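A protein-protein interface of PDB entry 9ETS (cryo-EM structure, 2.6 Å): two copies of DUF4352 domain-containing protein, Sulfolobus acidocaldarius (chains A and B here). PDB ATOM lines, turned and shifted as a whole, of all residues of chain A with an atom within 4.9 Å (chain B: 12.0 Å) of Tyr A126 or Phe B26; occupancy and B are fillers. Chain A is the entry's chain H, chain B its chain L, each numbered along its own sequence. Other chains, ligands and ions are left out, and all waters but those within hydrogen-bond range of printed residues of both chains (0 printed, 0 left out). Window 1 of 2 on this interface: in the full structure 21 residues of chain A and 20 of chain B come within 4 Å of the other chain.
The backbone carbonyl oxygen (O) of Phe B26 lies within hydrogen-bond range of the side-chain hydroxyl (OH) of Tyr A126, 2.7 Å away.
O of Gln A35 lies close to OE1 of Gln A131 (3.3 Å). The backbone NH of Thr A76 sits at hydrogen-bond distance from the backbone carbonyl oxygen of Tyr A126, 2.8 Å away. The backbone carbonyl oxygen of Ser A77 sits at hydrogen-bond distance from the backbone NH of Tyr A126 (2.9 Å). The backbone carbonyl oxygen (O) of Ile B29 lies within hydrogen-bond range of the side-chain hydroxyl (OG) of Ser B33 (2.7 Å).
Among the printed residues, pairs that only touch across the chains: Tyr A126 with Pro B30, Gly A132 with Phe B26, Thr A124 with Pro B30, Thr A124 with Ile B29, Gly A130 with Leu B23, Gln A35 with Leu B23, Tyr A126 with Gly B27 and Gln A131 with Phe B26.
Of chain B, only Phe B26 (2.7 Å), Gly B27 (3.8 Å) and Pro B30 (3.3 Å) come within 4 Å of Tyr A126. Of the printed residues of chain A, Phe B26 touches Tyr A126 (2.7 Å), Gln A131 (3.98 Å) and Gly A132 (3.3 Å). Of the printed residues of chain B, Gln A35 touches Leu B23. No residue of chain B comes within 4 Å of Val A75. No residue of chain B comes within 4 Å of Ser A77. Of chain B, only Ile B29 and Pro B30 come within 4 Å of Thr A124. Ile A125 touches none of the printed residues of chain B. No residue of chain B comes within 4 Å of Phe A127. No residue of chain B comes within 4 Å of Ser A128. Gly A130 touches just one residue of chain B: Leu B23 (3.6 Å). Of the printed residues of chain B, Gly A132 touches Phe B26. Of the printed residues of chain B, Gln A131 touches Phe B26 (3.98 Å). Of the printed residues of chain A, Ile B29 touches Thr A124 (3.6 Å). Printed residues of chain A within 4 Å of Pro B30: Thr A124 (3.5 Å) and Tyr A126 (3.3 Å). Ile B32 touches none of the printed residues of chain A. Val B21 touches none of the printed residues of chain A. The nearest residue of chain B that does not touch Tyr A126 is Ile B29 (5.0 Å). The nearest printed residue of chain A that does not touch Phe B26 is Gly A130 (4.3 Å). The nearest printed residue of chain A that does not touch Gly B27 is Gly A130 (6.7 Å).
Printed residues of chain A that touch a printed residue of chain B: Gln A35, Thr A124, Tyr A126, Gly A130, Gln A131 and Gly A132. Of the 19 printed residues of chain B, 5 touch a printed residue of chain A. Hydrophobic or aromatic side chains of chain B within 4 Å of the printed part of chain A: Leu B23, Phe B26, Ile B29 and Pro B30. Among the printed residues, 9 pairs touch across the chains. Among the printed residues, no Asp or Glu carboxylate lies within 4 Å of a Lys or Arg side-chain nitrogen of the other chain.
No position is printed for both chains. Of the 9 pairs that touch across the chains among the printed residues, none has its exchanged pair printed and touching as well.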
ATOM      1  N   GLN A  35       8.721   6.038  12.898  1.00  0.00           N
ATOM      2  CA  GLN A  35       7.395   6.564  13.212  1.00  0.00           C
ATOM      3  C   GLN A  35       7.100   7.880  12.479  1.00  0.00           C
ATOM      4  O   GLN A  35       5.939   8.262  12.354  1.00  0.00           O
ATOM      5  CB  GLN A  35       7.294   6.771  14.725  1.00  0.00           C
ATOM      6  CG  GLN A  35       5.869   6.773  15.264  1.00  0.00           C
ATOM      7  CD  GLN A  35       5.159   5.456  15.064  1.00  0.00           C
ATOM      8  OE1 GLN A  35       5.765   4.386  15.097  1.00  0.00           O
ATOM      9  NE2 GLN A  35       3.854   5.523  14.844  1.00  0.00           N
ATOM     10  N   SER A  74       2.147   1.947   3.343  1.00  0.00           N
ATOM     11  CA  SER A  74       0.835   1.982   2.699  1.00  0.00           C
ATOM     12  C   SER A  74      -0.251   2.646   3.559  1.00  0.00           C
ATOM     13  O   SER A  74      -0.167   2.684   4.784  1.00  0.00           O
ATOM     14  CB  SER A  74       0.429   0.593   2.263  1.00  0.00           C
ATOM     15  OG  SER A  74       0.253  -0.255   3.393  1.00  0.00           O
ATOM     16  N   VAL A  75      -1.294   3.163   2.894  1.00  0.00           N
ATOM     17  CA  VAL A  75      -2.436   3.785   3.551  1.00  0.00           C
ATOM     18  C   VAL A  75      -3.309   2.703   4.192  1.00  0.00           C
ATOM     19  O   VAL A  75      -3.872   1.866   3.493  1.00  0.00           O
ATOM     20  CB  VAL A  75      -3.243   4.631   2.545  1.00  0.00           C
ATOM     21  CG1 VAL A  75      -4.556   5.136   3.127  1.00  0.00           C
ATOM     22  CG2 VAL A  75      -2.428   5.785   1.999  1.00  0.00           C
ATOM     23  N   THR A  76      -3.462   2.736   5.524  1.00  0.00           N
ATOM     24  CA  THR A  76      -4.295   1.767   6.227  1.00  0.00           C
ATOM     25  C   THR A  76      -5.749   2.224   6.337  1.00  0.00           C
ATOM     26  O   THR A  76      -6.648   1.394   6.192  1.00  0.00           O
ATOM     27  CB  THR A  76      -3.751   1.401   7.613  1.00  0.00           C
ATOM     28  OG1 THR A  76      -3.772   2.532   8.480  1.00  0.00           O
ATOM     29  CG2 THR A  76      -2.354   0.833   7.571  1.00  0.00           C
ATOM     30  N   SER A  77      -5.971   3.516   6.623  1.00  0.00           N
ATOM     31  CA  SER A  77      -7.307   4.064   6.808  1.00  0.00           C
ATOM     32  C   SER A  77      -7.316   5.576   6.596  1.00  0.00           C
ATOM     33  O   SER A  77      -6.271   6.221   6.609  1.00  0.00           O
ATOM     34  CB  SER A  77      -7.886   3.688   8.151  1.00  0.00           C
ATOM     35  OG  SER A  77      -7.213   4.357   9.204  1.00  0.00           O
ATOM     36  N   THR A 124      -7.566  13.013   7.710  1.00  0.00           N
ATOM     37  CA  THR A 124      -6.364  12.461   8.315  1.00  0.00           C
ATOM     38  C   THR A 124      -6.140  11.089   7.702  1.00  0.00           C
ATOM     39  O   THR A 124      -7.038  10.251   7.724  1.00  0.00           O
ATOM     40  CB  THR A 124      -6.439  12.326   9.840  1.00  0.00           C
ATOM     41  OG1 THR A 124      -7.477  11.406  10.168  1.00  0.00           O
ATOM     42  CG2 THR A 124      -6.710  13.631  10.551  1.00  0.00           C
ATOM     43  N   ILE A 125      -4.940  10.874   7.152  1.00  0.00           N
ATOM     44  CA  ILE A 125      -4.597   9.598   6.551  1.00  0.00           C
ATOM     45  C   ILE A 125      -3.712   8.856   7.550  1.00  0.00           C
ATOM     46  O   ILE A 125      -2.768   9.443   8.067  1.00  0.00           O
ATOM     47  CB  ILE A 125      -3.920   9.786   5.173  1.00  0.00           C
ATOM     48  CG1 ILE A 125      -4.718  10.697   4.235  1.00  0.00           C
ATOM     49  CG2 ILE A 125      -3.682   8.438   4.519  1.00  0.00           C
ATOM     50  CD1 ILE A 125      -4.294  12.145   4.254  1.00  0.00           C
ATOM     51  N   TYR A 126      -4.021   7.579   7.822  1.00  0.00           N
ATOM     52  CA  TYR A 126      -3.210   6.755   8.701  1.00  0.00           C
ATOM     53  C   TYR A 126      -2.420   5.753   7.874  1.00  0.00           C
ATOM     54  O   TYR A 126      -2.988   4.940   7.152  1.00  0.00           O
ATOM     55  CB  TYR A 126      -4.087   6.051   9.734  1.00  0.00           C
ATOM     56  CG  TYR A 126      -4.621   6.986  10.784  1.00  0.00           C
ATOM     57  CD1 TYR A 126      -3.821   7.400  11.841  1.00  0.00           C
ATOM     58  CD2 TYR A 126      -5.905   7.503  10.691  1.00  0.00           C
ATOM     59  CE1 TYR A 126      -4.290   8.292  12.794  1.00  0.00           C
ATOM     60  CE2 TYR A 126      -6.394   8.386  11.641  1.00  0.00           C
ATOM     61  CZ  TYR A 126      -5.584   8.782  12.694  1.00  0.00           C
ATOM     62  OH  TYR A 126      -6.065   9.658  13.627  1.00  0.00           O
ATOM     63  N   PHE A 127      -1.097   5.786   8.029  1.00  0.00           N
ATOM     64  CA  PHE A 127      -0.187   4.917   7.296  1.00  0.00           C
ATOM     65  C   PHE A 127       0.200   3.697   8.134  1.00  0.00           C
ATOM     66  O   PHE A 127      -0.025   3.678   9.342  1.00  0.00           O
ATOM     67  CB  PHE A 127       1.017   5.752   6.863  1.00  0.00           C
ATOM     68  CG  PHE A 127       0.638   6.890   5.948  1.00  0.00           C
ATOM     69  CD1 PHE A 127       0.504   6.683   4.582  1.00  0.00           C
ATOM     70  CD2 PHE A 127       0.369   8.157   6.455  1.00  0.00           C
ATOM     71  CE1 PHE A 127       0.143   7.729   3.739  1.00  0.00           C
ATOM     72  CE2 PHE A 127      -0.007   9.201   5.619  1.00  0.00           C
ATOM     73  CZ  PHE A 127      -0.121   8.982   4.261  1.00  0.00           C
ATOM     74  N   SER A 128       0.830   2.691   7.508  1.00  0.00           N
ATOM     75  CA  SER A 128       1.163   1.423   8.159  1.00  0.00           C
ATOM     76  C   SER A 128       2.155   1.544   9.328  1.00  0.00           C
ATOM     77  O   SER A 128       2.323   0.587  10.087  1.00  0.00           O
ATOM     78  CB  SER A 128       1.552   0.378   7.143  1.00  0.00           C
ATOM     79  OG  SER A 128       2.750   0.739   6.474  1.00  0.00           O
ATOM     80  N   GLY A 130       1.342   3.368  11.788  1.00  0.00           N
ATOM     81  CA  GLY A 130       0.478   3.916  12.828  1.00  0.00           C
ATOM     82  C   GLY A 130       0.490   5.449  12.886  1.00  0.00           C
ATOM     83  O   GLY A 130      -0.331   6.044  13.590  1.00  0.00           O
ATOM     84  N   GLN A 131       1.393   6.086  12.121  1.00  0.00           N
ATOM     85  CA  GLN A 131       1.470   7.537  11.970  1.00  0.00           C
ATOM     86  C   GLN A 131       0.224   8.074  11.260  1.00  0.00           C
ATOM     87  O   GLN A 131      -0.193   7.529  10.240  1.00  0.00           O
ATOM     88  CB  GLN A 131       2.715   7.882  11.152  1.00  0.00           C
ATOM     89  CG  GLN A 131       3.023   9.373  11.122  1.00  0.00           C
ATOM     90  CD  GLN A 131       4.060   9.777  10.101  1.00  0.00           C
ATOM     91  OE1 GLN A 131       4.686   8.955   9.434  1.00  0.00           O
ATOM     92  NE2 GLN A 131       4.248  11.078   9.944  1.00  0.00           N
ATOM     93  N   GLY A 132      -0.350   9.163  11.793  1.00  0.00           N
ATOM     94  CA  GLY A 132      -1.449   9.859  11.144  1.00  0.00           C
ATOM     95  C   GLY A 132      -1.028  11.261  10.709  1.00  0.00           C
ATOM     96  O   GLY A 132      -0.391  11.978  11.474  1.00  0.00           O
ATOM     97  N   ILE B  16       7.349   0.950  25.164  1.00  0.00           N
ATOM     98  CA  ILE B  16       5.964   0.542  24.958  1.00  0.00           C
ATOM     99  C   ILE B  16       4.994   1.654  25.366  1.00  0.00           C
ATOM    100  O   ILE B  16       4.143   2.050  24.571  1.00  0.00           O
ATOM    101  CB  ILE B  16       5.668  -0.783  25.690  1.00  0.00           C
ATOM    102  CG1 ILE B  16       6.477  -1.939  25.103  1.00  0.00           C
ATOM    103  CG2 ILE B  16       4.174  -1.100  25.712  1.00  0.00           C
ATOM    104  CD1 ILE B  16       6.639  -3.115  26.048  1.00  0.00           C
ATOM    105  N   ILE B  17       5.129   2.175  26.592  1.00  0.00           N
ATOM    106  CA  ILE B  17       4.219   3.182  27.127  1.00  0.00           C
ATOM    107  C   ILE B  17       4.368   4.514  26.382  1.00  0.00           C
ATOM    108  O   ILE B  17       3.371   5.162  26.092  1.00  0.00           O
ATOM    109  CB  ILE B  17       4.349   3.297  28.663  1.00  0.00           C
ATOM    110  CG1 ILE B  17       4.004   1.964  29.333  1.00  0.00           C
ATOM    111  CG2 ILE B  17       3.473   4.419  29.211  1.00  0.00           C
ATOM    112  CD1 ILE B  17       4.414   1.841  30.785  1.00  0.00           C
ATOM    113  N   ALA B  18       5.592   4.904  26.013  1.00  0.00           N
ATOM    114  CA  ALA B  18       5.822   6.117  25.237  1.00  0.00           C
ATOM    115  C   ALA B  18       5.191   6.033  23.840  1.00  0.00           C
ATOM    116  O   ALA B  18       4.495   6.961  23.432  1.00  0.00           O
ATOM    117  CB  ALA B  18       7.294   6.438  25.183  1.00  0.00           C
ATOM    118  N   ILE B  19       5.377   4.919  23.124  1.00  0.00           N
ATOM    119  CA  ILE B  19       4.763   4.735  21.812  1.00  0.00           C
ATOM    120  C   ILE B  19       3.233   4.710  21.910  1.00  0.00           C
ATOM    121  O   ILE B  19       2.577   5.326  21.078  1.00  0.00           O
ATOM    122  CB  ILE B  19       5.367   3.524  21.073  1.00  0.00           C
ATOM    123  CG1 ILE B  19       6.825   3.817  20.712  1.00  0.00           C
ATOM    124  CG2 ILE B  19       4.553   3.146  19.839  1.00  0.00           C
ATOM    125  CD1 ILE B  19       7.584   2.639  20.142  1.00  0.00           C
ATOM    126  N   ALA B  20       2.663   4.086  22.952  1.00  0.00           N
ATOM    127  CA  ALA B  20       1.223   4.097  23.179  1.00  0.00           C
ATOM    128  C   ALA B  20       0.654   5.520  23.288  1.00  0.00           C
ATOM    129  O   ALA B  20      -0.395   5.806  22.707  1.00  0.00           O
ATOM    130  CB  ALA B  20       0.895   3.254  24.385  1.00  0.00           C
ATOM    131  N   VAL B  21       1.352   6.429  23.979  1.00  0.00           N
ATOM    132  CA  VAL B  21       0.939   7.823  24.121  1.00  0.00           C
ATOM    133  C   VAL B  21       1.100   8.601  22.808  1.00  0.00           C
ATOM    134  O   VAL B  21       0.252   9.434  22.486  1.00  0.00           O
ATOM    135  CB  VAL B  21       1.651   8.490  25.317  1.00  0.00           C
ATOM    136  CG1 VAL B  21       1.481  10.005  25.373  1.00  0.00           C
ATOM    137  CG2 VAL B  21       1.189   7.866  26.622  1.00  0.00           C
ATOM    138  N   VAL B  22       2.138   8.321  22.011  1.00  0.00           N
ATOM    139  CA  VAL B  22       2.308   8.945  20.701  1.00  0.00           C
ATOM    140  C   VAL B  22       1.189   8.532  19.738  1.00  0.00           C
ATOM    141  O   VAL B  22       0.615   9.384  19.061  1.00  0.00           O
ATOM    142  CB  VAL B  22       3.711   8.658  20.138  1.00  0.00           C
ATOM    143  CG1 VAL B  22       3.865   9.067  18.682  1.00  0.00           C
ATOM    144  CG2 VAL B  22       4.766   9.343  20.984  1.00  0.00           C
ATOM    145  N   LEU B  23       0.838   7.237  19.706  1.00  0.00           N
ATOM    146  CA  LEU B  23      -0.287   6.743  18.920  1.00  0.00           C
ATOM    147  C   LEU B  23      -1.610   7.357  19.386  1.00  0.00           C
ATOM    148  O   LEU B  23      -2.446   7.705  18.553  1.00  0.00           O
ATOM    149  CB  LEU B  23      -0.339   5.214  18.967  1.00  0.00           C
ATOM    150  CG  LEU B  23       0.792   4.478  18.252  1.00  0.00           C
ATOM    151  CD1 LEU B  23       0.702   2.989  18.531  1.00  0.00           C
ATOM    152  CD2 LEU B  23       0.775   4.739  16.751  1.00  0.00           C
ATOM    153  N   PHE B  24      -1.793   7.532  20.703  1.00  0.00           N
ATOM    154  CA  PHE B  24      -2.950   8.223  21.251  1.00  0.00           C
ATOM    155  C   PHE B  24      -3.050   9.662  20.736  1.00  0.00           C
ATOM    156  O   PHE B  24      -4.123  10.077  20.296  1.00  0.00           O
ATOM    157  CB  PHE B  24      -2.945   8.150  22.778  1.00  0.00           C
ATOM    158  CG  PHE B  24      -4.066   8.922  23.427  1.00  0.00           C
ATOM    159  CD1 PHE B  24      -5.328   8.358  23.561  1.00  0.00           C
ATOM    160  CD2 PHE B  24      -3.876  10.222  23.880  1.00  0.00           C
ATOM    161  CE1 PHE B  24      -6.369   9.065  24.150  1.00  0.00           C
ATOM    162  CE2 PHE B  24      -4.919  10.932  24.465  1.00  0.00           C
ATOM    163  CZ  PHE B  24      -6.162  10.351  24.600  1.00  0.00           C
ATOM    164  N   ALA B  25      -1.939  10.413  20.742  1.00  0.00           N
ATOM    165  CA  ALA B  25      -1.915  11.783  20.235  1.00  0.00           C
ATOM    166  C   ALA B  25      -2.309  11.865  18.752  1.00  0.00           C
ATOM    167  O   ALA B  25      -3.123  12.713  18.394  1.00  0.00           O
ATOM    168  CB  ALA B  25      -0.582  12.419  20.531  1.00  0.00           C
ATOM    169  N   PHE B  26      -1.811  10.965  17.891  1.00  0.00           N
ATOM    170  CA  PHE B  26      -2.277  10.877  16.509  1.00  0.00           C
ATOM    171  C   PHE B  26      -3.766  10.517  16.396  1.00  0.00           C
ATOM    172  O   PHE B  26      -4.411  10.884  15.418  1.00  0.00           O
ATOM    173  CB  PHE B  26      -1.457   9.853  15.722  1.00  0.00           C
ATOM    174  CG  PHE B  26      -0.038  10.250  15.395  1.00  0.00           C
ATOM    175  CD1 PHE B  26       0.221  11.408  14.672  1.00  0.00           C
ATOM    176  CD2 PHE B  26       1.040   9.456  15.776  1.00  0.00           C
ATOM    177  CE1 PHE B  26       1.520  11.775  14.347  1.00  0.00           C
ATOM    178  CE2 PHE B  26       2.339   9.821  15.442  1.00  0.00           C
ATOM    179  CZ  PHE B  26       2.577  10.982  14.738  1.00  0.00           C
ATOM    180  N   GLY B  27      -4.324   9.801  17.381  1.00  0.00           N
ATOM    181  CA  GLY B  27      -5.737   9.449  17.417  1.00  0.00           C
ATOM    182  C   GLY B  27      -6.680  10.607  17.767  1.00  0.00           C
ATOM    183  O   GLY B  27      -7.867  10.520  17.472  1.00  0.00           O
ATOM    184  N   LEU B  28      -6.177  11.702  18.359  1.00  0.00           N
ATOM    185  CA  LEU B  28      -6.990  12.870  18.687  1.00  0.00           C
ATOM    186  C   LEU B  28      -7.292  13.734  17.463  1.00  0.00           C
ATOM    187  O   LEU B  28      -8.319  14.414  17.425  1.00  0.00           O
ATOM    188  CB  LEU B  28      -6.267  13.736  19.718  1.00  0.00           C
ATOM    189  CG  LEU B  28      -6.143  13.156  21.119  1.00  0.00           C
ATOM    190  CD1 LEU B  28      -5.293  14.089  21.951  1.00  0.00           C
ATOM    191  CD2 LEU B  28      -7.514  12.991  21.768  1.00  0.00           C
ATOM    192  N   ILE B  29      -6.394  13.733  16.473  1.00  0.00           N
ATOM    193  CA  ILE B  29      -6.402  14.699  15.381  1.00  0.00           C
ATOM    194  C   ILE B  29      -7.747  14.748  14.643  1.00  0.00           C
ATOM    195  O   ILE B  29      -8.221  15.845  14.374  1.00  0.00           O
ATOM    196  CB  ILE B  29      -5.166  14.507  14.476  1.00  0.00           C
ATOM    197  CG1 ILE B  29      -3.880  14.731  15.281  1.00  0.00           C
ATOM    198  CG2 ILE B  29      -5.206  15.403  13.245  1.00  0.00           C
ATOM    199  CD1 ILE B  29      -2.589  14.477  14.518  1.00  0.00           C
ATOM    200  N   PRO B  30      -8.430  13.625  14.302  1.00  0.00           N
ATOM    201  CA  PRO B  30      -9.731  13.674  13.639  1.00  0.00           C
ATOM    202  C   PRO B  30     -10.845  14.347  14.430  1.00  0.00           C
ATOM    203  O   PRO B  30     -11.739  14.924  13.824  1.00  0.00           O
ATOM    204  CB  PRO B  30     -10.110  12.201  13.432  1.00  0.00           C
ATOM    205  CG  PRO B  30      -8.785  11.498  13.403  1.00  0.00           C
ATOM    206  CD  PRO B  30      -7.982  12.241  14.446  1.00  0.00           C
ATOM    207  N   GLY B  31     -10.803  14.268  15.766  1.00  0.00           N
ATOM    208  CA  GLY B  31     -11.834  14.858  16.610  1.00  0.00           C
ATOM    209  C   GLY B  31     -11.678  16.372  16.748  1.00  0.00           C
ATOM    210  O   GLY B  31     -12.654  17.115  16.651  1.00  0.00           O
ATOM    211  N   ILE B  32     -10.438  16.826  16.957  1.00  0.00           N
ATOM    212  CA  ILE B  32     -10.130  18.226  17.219  1.00  0.00           C
ATOM    213  C   ILE B  32     -10.073  19.057  15.932  1.00  0.00           C
ATOM    214  O   ILE B  32     -10.310  20.261  15.984  1.00  0.00           O
ATOM    215  CB  ILE B  32      -8.830  18.359  18.036  1.00  0.00           C
ATOM    216  CG1 ILE B  32      -7.601  17.964  17.207  1.00  0.00           C
ATOM    217  CG2 ILE B  32      -8.948  17.582  19.339  1.00  0.00           C
ATOM    218  CD1 ILE B  32      -6.284  18.017  17.937  1.00  0.00           C
ATOM    219  N   SER B  33      -9.699  18.445  14.799  1.00  0.00           N
ATOM    220  CA  SER B  33      -9.548  19.149  13.534  1.00  0.00           C
ATOM    221  C   SER B  33     -10.726  18.823  12.616  1.00  0.00           C
ATOM    222  O   SER B  33     -10.982  17.666  12.285  1.00  0.00           O
ATOM    223  CB  SER B  33      -8.188  18.909  12.898  1.00  0.00           C
ATOM    224  OG  SER B  33      -8.053  17.599  12.367  1.00  0.00           O
ATOM    225  N   ASN B  34     -11.469  19.866  12.241  1.00  0.00           N
ATOM    226  CA  ASN B  34     -12.789  19.718  11.666  1.00  0.00           C
ATOM    227  C   ASN B  34     -13.078  21.027  10.941  1.00  0.00           C
ATOM    228  O   ASN B  34     -13.509  21.987  11.574  1.00  0.00           O
ATOM    229  CB  ASN B  34     -13.777  19.391  12.793  1.00  0.00           C
ATOM    230  CG  ASN B  34     -15.176  19.047  12.336  1.00  0.00           C
ATOM    231  OD1 ASN B  34     -15.655  19.533  11.317  1.00  0.00           O
ATOM    232  ND2 ASN B  34     -15.858  18.213  13.104  1.00  0.00           N
